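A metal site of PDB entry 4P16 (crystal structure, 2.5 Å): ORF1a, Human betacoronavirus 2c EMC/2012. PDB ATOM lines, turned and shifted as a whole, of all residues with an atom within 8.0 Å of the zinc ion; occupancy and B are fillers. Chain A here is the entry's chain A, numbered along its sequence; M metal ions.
The guanidinium group (NH2) of Arg 238 lies close to the side-chain sulfur (SG) of Cys 232 (3.6 Å).
The side-chain sulfur of Cys 197 sits close to the backbone NH of Val 199, 3.4 Å away.
SG of Cys 234 sits close to N of Gly 236 (3.3 Å).
The nearest printed residue that does not touch the zinc ion is Val 199 (4.5 Å).
The zinc ion is bound by SG of Cys 197 (2.2 Å), SG of Cys 200 (2.3 Å), SG of Cys 234 (2.3 Å) and SG of Cys 232 (2.4 Å).
The zinc ion has four donor atoms within binding distance.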
ATOM      1  N   TRP A 196      -3.969 -25.864   8.882  1.00  0.00           N
ATOM      2  CA  TRP A 196      -4.362 -26.183  10.263  1.00  0.00           C
ATOM      3  C   TRP A 196      -3.833 -27.495  10.831  1.00  0.00           C
ATOM      4  O   TRP A 196      -3.528 -28.446  10.106  1.00  0.00           O
ATOM      5  CB  TRP A 196      -5.908 -26.154  10.400  1.00  0.00           C
ATOM      6  CG  TRP A 196      -6.611 -27.409   9.954  1.00  0.00           C
ATOM      7  CD1 TRP A 196      -7.070 -28.425  10.735  1.00  0.00           C
ATOM      8  CD2 TRP A 196      -6.886 -27.793   8.585  1.00  0.00           C
ATOM      9  NE1 TRP A 196      -7.608 -29.423   9.950  1.00  0.00           N
ATOM     10  CE2 TRP A 196      -7.550 -29.042   8.631  1.00  0.00           C
ATOM     11  CE3 TRP A 196      -6.690 -27.179   7.333  1.00  0.00           C
ATOM     12  CZ2 TRP A 196      -8.020 -29.687   7.484  1.00  0.00           C
ATOM     13  CZ3 TRP A 196      -7.121 -27.836   6.186  1.00  0.00           C
ATOM     14  CH2 TRP A 196      -7.782 -29.078   6.267  1.00  0.00           C
ATOM     15  N   CYS A 197      -3.791 -27.518  12.159  1.00  0.00           N
ATOM     16  CA  CYS A 197      -3.538 -28.655  13.020  1.00  0.00           C
ATOM     17  C   CYS A 197      -4.691 -28.630  14.009  1.00  0.00           C
ATOM     18  O   CYS A 197      -4.960 -27.582  14.594  1.00  0.00           O
ATOM     19  CB  CYS A 197      -2.202 -28.519  13.758  1.00  0.00           C
ATOM     20  SG  CYS A 197      -1.942 -29.768  15.054  1.00  0.00           S
ATOM     21  N   ASN A 198      -5.328 -29.779  14.229  1.00  0.00           N
ATOM     22  CA  ASN A 198      -6.417 -29.904  15.201  1.00  0.00           C
ATOM     23  C   ASN A 198      -6.028 -29.541  16.648  1.00  0.00           C
ATOM     24  O   ASN A 198      -6.910 -29.277  17.465  1.00  0.00           O
ATOM     25  CB  ASN A 198      -7.025 -31.297  15.115  1.00  0.00           C
ATOM     26  CG  ASN A 198      -7.633 -31.592  13.761  1.00  0.00           C
ATOM     27  OD1 ASN A 198      -7.496 -32.690  13.236  1.00  0.00           O
ATOM     28  ND2 ASN A 198      -8.303 -30.604  13.154  1.00  0.00           N
ATOM     29  N   VAL A 199      -4.707 -29.470  16.937  1.00  0.00           N
ATOM     30  CA  VAL A 199      -4.114 -29.104  18.231  1.00  0.00           C
ATOM     31  C   VAL A 199      -3.525 -27.655  18.186  1.00  0.00           C
ATOM     32  O   VAL A 199      -3.811 -26.863  19.093  1.00  0.00           O
ATOM     33  CB  VAL A 199      -3.019 -30.111  18.689  1.00  0.00           C
ATOM     34  CG1 VAL A 199      -2.664 -29.916  20.157  1.00  0.00           C
ATOM     35  CG2 VAL A 199      -3.388 -31.563  18.418  1.00  0.00           C
ATOM     36  N   CYS A 200      -2.700 -27.324  17.168  1.00  0.00           N
ATOM     37  CA  CYS A 200      -2.010 -26.025  17.135  1.00  0.00           C
ATOM     38  C   CYS A 200      -2.867 -24.848  16.742  1.00  0.00           C
ATOM     39  O   CYS A 200      -2.575 -23.732  17.158  1.00  0.00           O
ATOM     40  CB  CYS A 200      -0.749 -26.093  16.279  1.00  0.00           C
ATOM     41  SG  CYS A 200       0.383 -27.396  16.781  1.00  0.00           S
ATOM     42  N   GLY A 201      -3.885 -25.090  15.930  1.00  0.00           N
ATOM     43  CA  GLY A 201      -4.773 -24.024  15.502  1.00  0.00           C
ATOM     44  C   GLY A 201      -4.853 -23.881  13.999  1.00  0.00           C
ATOM     45  O   GLY A 201      -4.163 -24.575  13.258  1.00  0.00           O
ATOM     46  N   VAL A 231       3.760 -33.487   8.390  1.00  0.00           N
ATOM     47  CA  VAL A 231       4.036 -33.514   9.834  1.00  0.00           C
ATOM     48  C   VAL A 231       3.952 -32.083  10.459  1.00  0.00           C
ATOM     49  O   VAL A 231       4.569 -31.155   9.933  1.00  0.00           O
ATOM     50  CB  VAL A 231       5.419 -34.188  10.095  1.00  0.00           C
ATOM     51  CG1 VAL A 231       5.910 -33.969  11.524  1.00  0.00           C
ATOM     52  CG2 VAL A 231       5.384 -35.673   9.754  1.00  0.00           C
ATOM     53  N   CYS A 232       3.209 -31.931  11.581  1.00  0.00           N
ATOM     54  CA  CYS A 232       3.131 -30.674  12.341  1.00  0.00           C
ATOM     55  C   CYS A 232       4.287 -30.619  13.356  1.00  0.00           C
ATOM     56  O   CYS A 232       4.809 -31.678  13.754  1.00  0.00           O
ATOM     57  CB  CYS A 232       1.787 -30.508  13.033  1.00  0.00           C
ATOM     58  SG  CYS A 232       1.513 -28.859  13.755  1.00  0.00           S
ATOM     59  N   GLN A 233       4.648 -29.387  13.805  1.00  0.00           N
ATOM     60  CA  GLN A 233       5.673 -29.203  14.839  1.00  0.00           C
ATOM     61  C   GLN A 233       5.350 -29.965  16.137  1.00  0.00           C
ATOM     62  O   GLN A 233       6.224 -30.625  16.673  1.00  0.00           O
ATOM     63  CB  GLN A 233       5.946 -27.723  15.113  1.00  0.00           C
ATOM     64  CG  GLN A 233       4.765 -26.908  15.618  1.00  0.00           C
ATOM     65  CD  GLN A 233       5.001 -26.480  17.043  1.00  0.00           C
ATOM     66  OE1 GLN A 233       5.675 -25.478  17.297  1.00  0.00           O
ATOM     67  NE2 GLN A 233       4.497 -27.261  17.997  1.00  0.00           N
ATOM     68  N   CYS A 234       4.068 -29.968  16.545  1.00  0.00           N
ATOM     69  CA  CYS A 234       3.545 -30.659  17.729  1.00  0.00           C
ATOM     70  C   CYS A 234       3.797 -32.171  17.705  1.00  0.00           C
ATOM     71  O   CYS A 234       3.799 -32.802  18.763  1.00  0.00           O
ATOM     72  CB  CYS A 234       2.071 -30.349  17.908  1.00  0.00           C
ATOM     73  SG  CYS A 234       0.986 -31.235  16.762  1.00  0.00           S
ATOM     74  N   GLY A 235       3.944 -32.740  16.513  1.00  0.00           N
ATOM     75  CA  GLY A 235       4.150 -34.164  16.283  1.00  0.00           C
ATOM     76  C   GLY A 235       2.993 -34.841  15.570  1.00  0.00           C
ATOM     77  O   GLY A 235       3.110 -35.995  15.135  1.00  0.00           O
ATOM     78  N   GLY A 236       1.871 -34.129  15.461  1.00  0.00           N
ATOM     79  CA  GLY A 236       0.666 -34.628  14.818  1.00  0.00           C
ATOM     80  C   GLY A 236       0.704 -34.398  13.326  1.00  0.00           C
ATOM     81  O   GLY A 236       1.780 -34.375  12.706  1.00  0.00           O
ATOM     82  N   GLU A 237      -0.489 -34.251  12.738  1.00  0.00           N
ATOM     83  CA  GLU A 237      -0.651 -33.980  11.316  1.00  0.00           C
ATOM     84  C   GLU A 237      -1.056 -32.523  11.115  1.00  0.00           C
ATOM     85  O   GLU A 237      -1.813 -31.963  11.918  1.00  0.00           O
ATOM     86  CB  GLU A 237      -1.672 -34.926  10.682  1.00  0.00           C
ATOM     87  CG  GLU A 237      -1.185 -36.354  10.536  1.00  0.00           C
ATOM     88  CD  GLU A 237      -2.244 -37.322  10.036  1.00  0.00           C
ATOM     89  OE1 GLU A 237      -1.937 -38.102   9.101  1.00  0.00           O
ATOM     90  OE2 GLU A 237      -3.378 -37.311  10.564  1.00  0.00           O
ATOM     91  N   ARG A 238      -0.501 -31.904  10.054  1.00  0.00           N
ATOM     92  CA  ARG A 238      -0.757 -30.531   9.610  1.00  0.00           C
ATOM     93  C   ARG A 238      -1.376 -30.649   8.208  1.00  0.00           C
ATOM     94  O   ARG A 238      -0.929 -31.479   7.399  1.00  0.00           O
ATOM     95  CB  ARG A 238       0.574 -29.729   9.542  1.00  0.00           C
ATOM     96  CG  ARG A 238       0.434 -28.247   9.224  1.00  0.00           C
ATOM     97  CD  ARG A 238       0.963 -27.363  10.332  1.00  0.00           C
ATOM     98  NE  ARG A 238       0.394 -26.020  10.256  1.00  0.00           N
ATOM     99  CZ  ARG A 238      -0.154 -25.363  11.274  1.00  0.00           C
ATOM    100  NH1 ARG A 238      -0.636 -24.142  11.102  1.00  0.00           N
ATOM    101  NH2 ARG A 238      -0.222 -25.932  12.480  1.00  0.00           N
HETATM  102 ZN    ZN M   1       0.172 -29.341  15.651  1.00  0.00          ZN
